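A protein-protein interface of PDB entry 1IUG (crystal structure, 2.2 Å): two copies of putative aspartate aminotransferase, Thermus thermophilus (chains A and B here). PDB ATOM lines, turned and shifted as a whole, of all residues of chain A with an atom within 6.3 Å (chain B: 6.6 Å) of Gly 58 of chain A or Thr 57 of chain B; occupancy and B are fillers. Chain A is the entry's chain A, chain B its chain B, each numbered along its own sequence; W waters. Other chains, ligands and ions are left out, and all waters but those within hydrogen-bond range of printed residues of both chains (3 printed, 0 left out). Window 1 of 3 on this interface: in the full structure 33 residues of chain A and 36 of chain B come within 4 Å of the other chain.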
ATOM      1  N   LEU A  56      -6.771  -7.796  12.141  1.00  0.00           N
ATOM      2  CA  LEU A  56      -7.150  -6.385  12.099  1.00  0.00           C
ATOM      3  C   LEU A  56      -7.237  -5.813  13.503  1.00  0.00           C
ATOM      4  O   LEU A  56      -7.694  -6.483  14.432  1.00  0.00           O
ATOM      5  CB  LEU A  56      -8.507  -6.218  11.410  1.00  0.00           C
ATOM      6  CG  LEU A  56      -8.695  -6.829  10.017  1.00  0.00           C
ATOM      7  CD1 LEU A  56     -10.096  -6.519   9.533  1.00  0.00           C
ATOM      8  CD2 LEU A  56      -7.667  -6.296   9.035  1.00  0.00           C
ATOM      9  N   THR A  57      -6.792  -4.574  13.657  1.00  0.00           N
ATOM     10  CA  THR A  57      -6.839  -3.916  14.950  1.00  0.00           C
ATOM     11  C   THR A  57      -8.182  -3.205  15.069  1.00  0.00           C
ATOM     12  O   THR A  57      -8.427  -2.188  14.420  1.00  0.00           O
ATOM     13  CB  THR A  57      -5.648  -2.949  15.123  1.00  0.00           C
ATOM     14  OG1 THR A  57      -4.431  -3.708  15.101  1.00  0.00           O
ATOM     15  CG2 THR A  57      -5.737  -2.202  16.452  1.00  0.00           C
ATOM     16  N   GLY A  58      -9.067  -3.807  15.853  1.00  0.00           N
ATOM     17  CA  GLY A  58     -10.404  -3.277  16.061  1.00  0.00           C
ATOM     18  C   GLY A  58     -11.279  -4.390  16.612  1.00  0.00           C
ATOM     19  O   GLY A  58     -10.790  -5.496  16.835  1.00  0.00           O
ATOM     20  N   SER A  59     -12.563  -4.121  16.833  1.00  0.00           N
ATOM     21  CA  SER A  59     -13.453  -5.146  17.369  1.00  0.00           C
ATOM     22  C   SER A  59     -13.938  -6.114  16.289  1.00  0.00           C
ATOM     23  O   SER A  59     -13.617  -5.960  15.108  1.00  0.00           O
ATOM     24  CB  SER A  59     -14.648  -4.517  18.094  1.00  0.00           C
ATOM     25  OG  SER A  59     -15.552  -3.919  17.179  1.00  0.00           O
ATOM     26  N   GLY A  60     -14.705  -7.117  16.716  1.00  0.00           N
ATOM     27  CA  GLY A  60     -15.232  -8.107  15.795  1.00  0.00           C
ATOM     28  C   GLY A  60     -16.079  -7.511  14.685  1.00  0.00           C
ATOM     29  O   GLY A  60     -16.014  -7.970  13.544  1.00  0.00           O
ATOM     30  N   THR A  61     -16.854  -6.478  15.016  1.00  0.00           N
ATOM     31  CA  THR A  61     -17.716  -5.806  14.045  1.00  0.00           C
ATOM     32  C   THR A  61     -16.905  -5.285  12.856  1.00  0.00           C
ATOM     33  O   THR A  61     -17.354  -5.369  11.706  1.00  0.00           O
ATOM     34  CB  THR A  61     -18.498  -4.641  14.704  1.00  0.00           C
ATOM     35  OG1 THR A  61     -19.280  -5.151  15.788  1.00  0.00           O
ATOM     36  CG2 THR A  61     -19.439  -3.978  13.702  1.00  0.00           C
ATOM     37  N   LEU A  62     -15.700  -4.786  13.134  1.00  0.00           N
ATOM     38  CA  LEU A  62     -14.819  -4.270  12.091  1.00  0.00           C
ATOM     39  C   LEU A  62     -14.483  -5.367  11.082  1.00  0.00           C
ATOM     40  O   LEU A  62     -14.448  -5.123   9.876  1.00  0.00           O
ATOM     41  CB  LEU A  62     -13.525  -3.718  12.699  1.00  0.00           C
ATOM     42  CG  LEU A  62     -12.521  -3.146  11.699  1.00  0.00           C
ATOM     43  CD1 LEU A  62     -13.085  -1.883  11.072  1.00  0.00           C
ATOM     44  CD2 LEU A  62     -11.211  -2.848  12.392  1.00  0.00           C
ATOM     45  N   ALA A  63     -14.223  -6.569  11.591  1.00  0.00           N
ATOM     46  CA  ALA A  63     -13.897  -7.721  10.750  1.00  0.00           C
ATOM     47  C   ALA A  63     -15.091  -8.110   9.873  1.00  0.00           C
ATOM     48  O   ALA A  63     -14.914  -8.533   8.730  1.00  0.00           O
ATOM     49  CB  ALA A  63     -13.466  -8.906  11.620  1.00  0.00           C
ATOM     50  N   SER A 183     -11.170 -11.325  19.240  1.00  0.00           N
ATOM     51  CA  SER A 183     -10.301 -11.804  20.302  1.00  0.00           C
ATOM     52  C   SER A 183     -10.900 -12.016  21.695  1.00  0.00           C
ATOM     53  O   SER A 183     -10.357 -12.804  22.473  1.00  0.00           O
ATOM     54  CB  SER A 183      -9.084 -10.880  20.410  1.00  0.00           C
ATOM     55  OG  SER A 183      -9.486  -9.542  20.653  1.00  0.00           O
ATOM     56  N   PRO A 191     -10.361  -7.514  24.353  1.00  0.00           N
ATOM     57  CA  PRO A 191     -10.994  -6.980  23.139  1.00  0.00           C
ATOM     58  C   PRO A 191      -9.933  -6.144  22.425  1.00  0.00           C
ATOM     59  O   PRO A 191      -9.030  -5.617  23.078  1.00  0.00           O
ATOM     60  CB  PRO A 191     -12.081  -6.058  23.696  1.00  0.00           C
ATOM     61  CG  PRO A 191     -12.365  -6.615  25.052  1.00  0.00           C
ATOM     62  CD  PRO A 191     -11.006  -6.976  25.562  1.00  0.00           C
ATOM     63  N   GLY A 192     -10.024  -6.023  21.104  1.00  0.00           N
ATOM     64  CA  GLY A 192      -9.043  -5.226  20.391  1.00  0.00           C
ATOM     65  C   GLY A 192      -8.594  -5.764  19.044  1.00  0.00           C
ATOM     66  O   GLY A 192      -7.983  -5.036  18.264  1.00  0.00           O
ATOM     67  N   LEU A 193      -8.859  -7.041  18.782  1.00  0.00           N
ATOM     68  CA  LEU A 193      -8.489  -7.649  17.508  1.00  0.00           C
ATOM     69  C   LEU A 193      -9.686  -8.300  16.827  1.00  0.00           C
ATOM     70  O   LEU A 193     -10.599  -8.801  17.487  1.00  0.00           O
ATOM     71  CB  LEU A 193      -7.393  -8.707  17.693  1.00  0.00           C
ATOM     72  CG  LEU A 193      -6.019  -8.294  18.220  1.00  0.00           C
ATOM     73  CD1 LEU A 193      -5.122  -9.525  18.287  1.00  0.00           C
ATOM     74  CD2 LEU A 193      -5.400  -7.229  17.315  1.00  0.00           C
ATOM     75  N   GLY A 194      -9.683  -8.241  15.499  1.00  0.00           N
ATOM     76  CA  GLY A 194     -10.721  -8.856  14.693  1.00  0.00           C
ATOM     77  C   GLY A 194      -9.985  -9.669  13.640  1.00  0.00           C
ATOM     78  O   GLY A 194      -8.870  -9.303  13.251  1.00  0.00           O
ATOM     79  N   TYR A 212      -8.901   2.041   5.571  1.00  0.00           N
ATOM     80  CA  TYR A 212      -8.319   1.359   6.726  1.00  0.00           C
ATOM     81  C   TYR A 212      -8.562  -0.141   6.644  1.00  0.00           C
ATOM     82  O   TYR A 212      -7.702  -0.929   7.038  1.00  0.00           O
ATOM     83  CB  TYR A 212      -8.924   1.887   8.028  1.00  0.00           C
ATOM     84  CG  TYR A 212      -8.374   1.254   9.295  1.00  0.00           C
ATOM     85  CD1 TYR A 212      -7.230   1.764   9.916  1.00  0.00           C
ATOM     86  CD2 TYR A 212      -9.025   0.176   9.903  1.00  0.00           C
ATOM     87  CE1 TYR A 212      -6.751   1.222  11.118  1.00  0.00           C
ATOM     88  CE2 TYR A 212      -8.556  -0.376  11.100  1.00  0.00           C
ATOM     89  CZ  TYR A 212      -7.419   0.155  11.702  1.00  0.00           C
ATOM     90  OH  TYR A 212      -6.964  -0.364  12.894  1.00  0.00           O
ATOM     91  N   ILE B  55     -13.391   7.848  21.717  1.00  0.00           N
ATOM     92  CA  ILE B  55     -12.412   6.774  21.785  1.00  0.00           C
ATOM     93  C   ILE B  55     -12.804   5.673  20.799  1.00  0.00           C
ATOM     94  O   ILE B  55     -13.880   5.085  20.900  1.00  0.00           O
ATOM     95  CB  ILE B  55     -12.316   6.186  23.213  1.00  0.00           C
ATOM     96  CG1 ILE B  55     -11.902   7.277  24.207  1.00  0.00           C
ATOM     97  CG2 ILE B  55     -11.304   5.049  23.252  1.00  0.00           C
ATOM     98  CD1 ILE B  55     -11.764   6.783  25.649  1.00  0.00           C
ATOM     99  N   LEU B  56     -11.941   5.431  19.824  1.00  0.00           N
ATOM    100  CA  LEU B  56     -12.188   4.409  18.809  1.00  0.00           C
ATOM    101  C   LEU B  56     -11.225   3.238  18.988  1.00  0.00           C
ATOM    102  O   LEU B  56     -10.058   3.433  19.305  1.00  0.00           O
ATOM    103  CB  LEU B  56     -11.999   4.996  17.407  1.00  0.00           C
ATOM    104  CG  LEU B  56     -12.819   6.210  16.968  1.00  0.00           C
ATOM    105  CD1 LEU B  56     -12.471   6.562  15.526  1.00  0.00           C
ATOM    106  CD2 LEU B  56     -14.301   5.914  17.092  1.00  0.00           C
ATOM    107  N   THR B  57     -11.724   2.022  18.814  1.00  0.00           N
ATOM    108  CA  THR B  57     -10.874   0.847  18.936  1.00  0.00           C
ATOM    109  C   THR B  57     -10.297   0.542  17.558  1.00  0.00           C
ATOM    110  O   THR B  57     -10.993   0.043  16.670  1.00  0.00           O
ATOM    111  CB  THR B  57     -11.639  -0.356  19.526  1.00  0.00           C
ATOM    112  OG1 THR B  57     -11.996  -0.058  20.881  1.00  0.00           O
ATOM    113  CG2 THR B  57     -10.760  -1.622  19.517  1.00  0.00           C
ATOM    114  N   GLY B  58      -9.035   0.926  17.389  1.00  0.00           N
ATOM    115  CA  GLY B  58      -8.314   0.749  16.142  1.00  0.00           C
ATOM    116  C   GLY B  58      -7.068   1.613  16.220  1.00  0.00           C
ATOM    117  O   GLY B  58      -6.845   2.258  17.240  1.00  0.00           O
ATOM    118  N   SER B  59      -6.256   1.646  15.169  1.00  0.00           N
ATOM    119  CA  SER B  59      -5.041   2.460  15.199  1.00  0.00           C
ATOM    120  C   SER B  59      -5.335   3.931  14.884  1.00  0.00           C
ATOM    121  O   SER B  59      -6.473   4.294  14.614  1.00  0.00           O
ATOM    122  CB  SER B  59      -3.988   1.899  14.237  1.00  0.00           C
ATOM    123  OG  SER B  59      -4.282   2.220  12.886  1.00  0.00           O
ATOM    124  N   LEU B  62      -7.243   4.929  11.674  1.00  0.00           N
ATOM    125  CA  LEU B  62      -8.695   4.782  11.717  1.00  0.00           C
ATOM    126  C   LEU B  62      -9.334   6.097  12.155  1.00  0.00           C
ATOM    127  O   LEU B  62     -10.333   6.532  11.586  1.00  0.00           O
ATOM    128  CB  LEU B  62      -9.099   3.670  12.693  1.00  0.00           C
ATOM    129  CG  LEU B  62     -10.604   3.395  12.810  1.00  0.00           C
ATOM    130  CD1 LEU B  62     -11.143   2.868  11.498  1.00  0.00           C
ATOM    131  CD2 LEU B  62     -10.872   2.399  13.910  1.00  0.00           C
ATOM    132  N   GLY B 192      -3.568   0.461  19.698  1.00  0.00           N
ATOM    133  CA  GLY B 192      -4.878  -0.165  19.740  1.00  0.00           C
ATOM    134  C   GLY B 192      -6.050   0.792  19.883  1.00  0.00           C
ATOM    135  O   GLY B 192      -7.200   0.373  19.751  1.00  0.00           O
ATOM    136  N   LEU B 193      -5.773   2.055  20.211  1.00  0.00           N
ATOM    137  CA  LEU B 193      -6.830   3.057  20.352  1.00  0.00           C
ATOM    138  C   LEU B 193      -6.570   4.268  19.466  1.00  0.00           C
ATOM    139  O   LEU B 193      -5.422   4.607  19.169  1.00  0.00           O
ATOM    140  CB  LEU B 193      -6.972   3.532  21.802  1.00  0.00           C
ATOM    141  CG  LEU B 193      -7.446   2.565  22.889  1.00  0.00           C
ATOM    142  CD1 LEU B 193      -7.474   3.300  24.221  1.00  0.00           C
ATOM    143  CD2 LEU B 193      -8.830   2.009  22.558  1.00  0.00           C
ATOM    144  N   GLY B 194      -7.657   4.878  19.016  1.00  0.00           N
ATOM    145  CA  GLY B 194      -7.584   6.065  18.184  1.00  0.00           C
ATOM    146  C   GLY B 194      -8.516   7.083  18.817  1.00  0.00           C
ATOM    147  O   GLY B 194      -9.525   6.713  19.422  1.00  0.00           O
ATOM    148  N   TYR B 212     -18.798   1.163  11.016  1.00  0.00           N
ATOM    149  CA  TYR B 212     -17.988   0.985  12.215  1.00  0.00           C
ATOM    150  C   TYR B 212     -17.533   2.353  12.734  1.00  0.00           C
ATOM    151  O   TYR B 212     -17.560   2.603  13.942  1.00  0.00           O
ATOM    152  CB  TYR B 212     -16.767   0.116  11.899  1.00  0.00           C
ATOM    153  CG  TYR B 212     -15.899  -0.202  13.096  1.00  0.00           C
ATOM    154  CD1 TYR B 212     -16.176  -1.299  13.913  1.00  0.00           C
ATOM    155  CD2 TYR B 212     -14.788   0.586  13.404  1.00  0.00           C
ATOM    156  CE1 TYR B 212     -15.363  -1.608  15.007  1.00  0.00           C
ATOM    157  CE2 TYR B 212     -13.972   0.286  14.496  1.00  0.00           C
ATOM    158  CZ  TYR B 212     -14.263  -0.811  15.292  1.00  0.00           C
ATOM    159  OH  TYR B 212     -13.450  -1.111  16.360  1.00  0.00           O
ATOM    160  N   GLU B 218     -21.284   6.643  17.896  1.00  0.00           N
ATOM    161  CA  GLU B 218     -20.382   6.678  19.043  1.00  0.00           C
ATOM    162  C   GLU B 218     -20.671   7.803  20.027  1.00  0.00           C
ATOM    163  O   GLU B 218     -20.588   7.605  21.236  1.00  0.00           O
ATOM    164  CB  GLU B 218     -18.928   6.768  18.570  1.00  0.00           C
ATOM    165  CG  GLU B 218     -18.403   5.508  17.887  1.00  0.00           C
ATOM    166  CD  GLU B 218     -18.179   4.341  18.841  1.00  0.00           C
ATOM    167  OE1 GLU B 218     -18.538   4.435  20.036  1.00  0.00           O
ATOM    168  OE2 GLU B 218     -17.636   3.311  18.387  1.00  0.00           O
ATOM    169  N   SER B 227     -19.963   2.598  24.339  1.00  0.00           N
ATOM    170  CA  SER B 227     -19.512   2.760  22.964  1.00  0.00           C
ATOM    171  C   SER B 227     -20.374   1.918  22.039  1.00  0.00           C
ATOM    172  O   SER B 227     -21.136   1.067  22.495  1.00  0.00           O
ATOM    173  CB  SER B 227     -18.028   2.400  22.819  1.00  0.00           C
ATOM    174  OG  SER B 227     -17.732   1.146  23.399  1.00  0.00           O
ATOM    175  N   TRP B 229     -19.554  -0.426  19.858  1.00  0.00           N
ATOM    176  CA  TRP B 229     -19.179  -1.844  19.891  1.00  0.00           C
ATOM    177  C   TRP B 229     -18.286  -2.091  21.104  1.00  0.00           C
ATOM    178  O   TRP B 229     -18.036  -1.176  21.891  1.00  0.00           O
ATOM    179  CB  TRP B 229     -18.420  -2.221  18.611  1.00  0.00           C
ATOM    180  CG  TRP B 229     -18.775  -1.371  17.425  1.00  0.00           C
ATOM    181  CD1 TRP B 229     -17.979  -0.438  16.820  1.00  0.00           C
ATOM    182  CD2 TRP B 229     -20.027  -1.341  16.729  1.00  0.00           C
ATOM    183  NE1 TRP B 229     -18.660   0.174  15.794  1.00  0.00           N
ATOM    184  CE2 TRP B 229     -19.919  -0.361  15.716  1.00  0.00           C
ATOM    185  CE3 TRP B 229     -21.230  -2.046  16.864  1.00  0.00           C
ATOM    186  CZ2 TRP B 229     -20.968  -0.069  14.842  1.00  0.00           C
ATOM    187  CZ3 TRP B 229     -22.277  -1.754  15.994  1.00  0.00           C
ATOM    188  CH2 TRP B 229     -22.137  -0.773  14.997  1.00  0.00           C
ATOM    189  N   THR B 230     -17.798  -3.316  21.266  1.00  0.00           N
ATOM    190  CA  THR B 230     -16.921  -3.612  22.394  1.00  0.00           C
ATOM    191  C   THR B 230     -15.605  -2.851  22.206  1.00  0.00           C
ATOM    192  O   THR B 230     -14.945  -2.987  21.176  1.00  0.00           O
ATOM    193  CB  THR B 230     -16.620  -5.127  22.515  1.00  0.00           C
ATOM    194  OG1 THR B 230     -17.846  -5.863  22.580  1.00  0.00           O
ATOM    195  CG2 THR B 230     -15.828  -5.412  23.772  1.00  0.00           C
ATOM    196  N   PRO B 231     -15.259  -1.971  23.159  1.00  0.00           N
ATOM    197  CA  PRO B 231     -14.020  -1.196  23.082  1.00  0.00           C
ATOM    198  C   PRO B 231     -12.867  -1.967  23.718  1.00  0.00           C
ATOM    199  O   PRO B 231     -13.095  -2.902  24.479  1.00  0.00           O
ATOM    200  CB  PRO B 231     -14.354   0.030  23.922  1.00  0.00           C
ATOM    201  CG  PRO B 231     -15.132  -0.573  25.044  1.00  0.00           C
ATOM    202  CD  PRO B 231     -16.070  -1.533  24.311  1.00  0.00           C
ATOM    203  N   ALA B 232     -11.635  -1.584  23.397  1.00  0.00           N
ATOM    204  CA  ALA B 232     -10.467  -2.220  23.997  1.00  0.00           C
ATOM    205  C   ALA B 232     -10.359  -1.613  25.401  1.00  0.00           C
ATOM    206  O   ALA B 232      -9.447  -0.835  25.697  1.00  0.00           O
ATOM    207  CB  ALA B 232      -9.219  -1.913  23.178  1.00  0.00           C
ATOM    208  N   ILE B 233     -11.325  -1.963  26.248  1.00  0.00           N
ATOM    209  CA  ILE B 233     -11.425  -1.461  27.613  1.00  0.00           C
ATOM    210  C   ILE B 233     -10.133  -1.526  28.441  1.00  0.00           C
ATOM    211  O   ILE B 233      -9.850  -0.602  29.208  1.00  0.00           O
ATOM    212  CB  ILE B 233     -12.615  -2.142  28.367  1.00  0.00           C
ATOM    213  CG1 ILE B 233     -12.921  -1.405  29.676  1.00  0.00           C
ATOM    214  CG2 ILE B 233     -12.325  -3.616  28.625  1.00  0.00           C
ATOM    215  CD1 ILE B 233     -13.414   0.016  29.476  1.00  0.00           C
ATOM    216  N   VAL B 236      -8.164   1.389  27.583  1.00  0.00           N
ATOM    217  CA  VAL B 236      -8.789   2.624  28.056  1.00  0.00           C
ATOM    218  C   VAL B 236      -8.367   2.870  29.505  1.00  0.00           C
ATOM    219  O   VAL B 236      -8.153   4.011  29.917  1.00  0.00           O
ATOM    220  CB  VAL B 236     -10.336   2.566  27.932  1.00  0.00           C
ATOM    221  CG1 VAL B 236     -10.981   3.806  28.565  1.00  0.00           C
ATOM    222  CG2 VAL B 236     -10.727   2.480  26.462  1.00  0.00           C
HETATM  223  O   HOH W   1     -14.899  -1.052  18.926  1.00  0.00           O
HETATM  224  O   HOH W   2     -12.484  -4.243  21.014  1.00  0.00           O
HETATM  225  O   HOH W   3      -7.145  -2.637  20.027  1.00  0.00           O
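Thr 57 of chain A touches Gly 58 of chain B, and with the chains exchanged Gly 58 of chain A touches Thr 57 of chain B. Thr 57 of chain A touches Gly 192 of chain B, but with the chains exchanged Gly 192 of chain A does not touch Thr 57 of chain B (4.1 Å). Gly 58 of chain A touches Tyr 212 of chain B, and with the chains exchanged Tyr 212 of chain A touches Gly 58 of chain B. Leu 62 of chain A touches Tyr 212 of chain B, and with the chains exchanged Tyr 212 of chain A touches Leu 62 of chain B. Positions printed for both chains: 56, 57, 58, 59, 62, 192, 193, 194 and 212. Of the 15 pairs that touch across the chains among the printed residues, 8 have their exchanged pair printed and touching as well.
OH of Tyr 212 of chain A sits at hydrogen-bond distance from O of Thr 57 of chain A (2.8 Å). The backbone NH (N) of Gly 58 of chain A is in hydrogen-bond range of the backbone carbonyl oxygen (O) of Gly 192 of chain A (2.9 Å). The backbone NH (N) of Gly 194 of chain A is in hydrogen-bond range of the backbone carbonyl oxygen (O) of Gly 58 of chain A, at 3.2 Å. OH of Tyr 212 of chain B sits at hydrogen-bond distance from O of Thr 57 of chain B, 2.7 Å away. N of Gly 194 of chain B sits at hydrogen-bond distance from O of Gly 58 of chain B. The side-chain hydroxyl (OG) of Ser 227 of chain B is in hydrogen-bond range of the backbone carbonyl oxygen (O) of Trp 229 of chain B.
N of Ser 59 of chain A is in hydrogen-bond range of OH of Tyr 212 of chain B (3.2 Å). The side-chain hydroxyl of Tyr 212 of chain A sits at hydrogen-bond distance from the backbone NH of Ser 59 of chain B, 3.1 Å away.
Gly 58 of chain A touches two residues of chain B. Printed residues of chain B within 4 Å of Pro 191 of chain A: Thr 230, Pro 231 and Ala 232. Thr 57 of chain B touches just one residue of chain A: Gly 58 (3.4 Å). Of the printed residues of chain A, Gly 192 of chain B touches Thr 57. Of the printed residues of chain A, Ala 232 of chain B touches Pro 191 (3.7 Å).
Hydrophobic or aromatic side chains of chain A that line the printed part of chain B: Leu 62, Pro 191 and Tyr 212. Of the 18 printed residues of chain B, 10 touch a printed residue of chain A. Among the printed residues, 15 pairs touch across the chains.
O of Thr 57 of chain A touches CA of Gly 58 of chain B, at 3.4 Å. Thr 57 of chain A touches Gly 192 of chain B (CG2 to CA, 3.96 Å). Gly 58 of chain A touches Thr 57 of chain B. Gly 58 of chain A touches Tyr 212 of chain B. OG of Ser 59 of chain A touches CB of Trp 229 of chain B (3.6 Å). Pro 191 of chain A touches Thr 230 of chain B (CB to CG2, 3.8 Å). O of Pro 231 of chain B touches CB of Pro 191 of chain A, 3.4 Å away. Pro 191 of chain A touches Ala 232 of chain B (O to CB, 3.7 Å). Tyr 212 of chain A touches Gly 58 of chain B. CD1 of Tyr 212 of chain A touches N of Leu 62 of chain B, 3.6 Å away.
Water W2 lies within hydrogen-bond range of the backbone carbonyl oxygen (O) of Thr 230 of chain B (2.8 Å) and the backbone NH (N) of Gly 192 of chain A (3.0 Å). Water W1 lies within hydrogen-bond range of the side-chain hydroxyl of Tyr 212 of chain B (2.9 Å), the backbone carbonyl oxygen of Thr 230 of chain B (3.0 Å) and the side-chain hydroxyl of Ser 59 of chain A (3.4 Å). Water W3 bridges O of Gly 192 of chain B (3.0 Å) and O of Gly 192 of chain A (3.1 Å).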
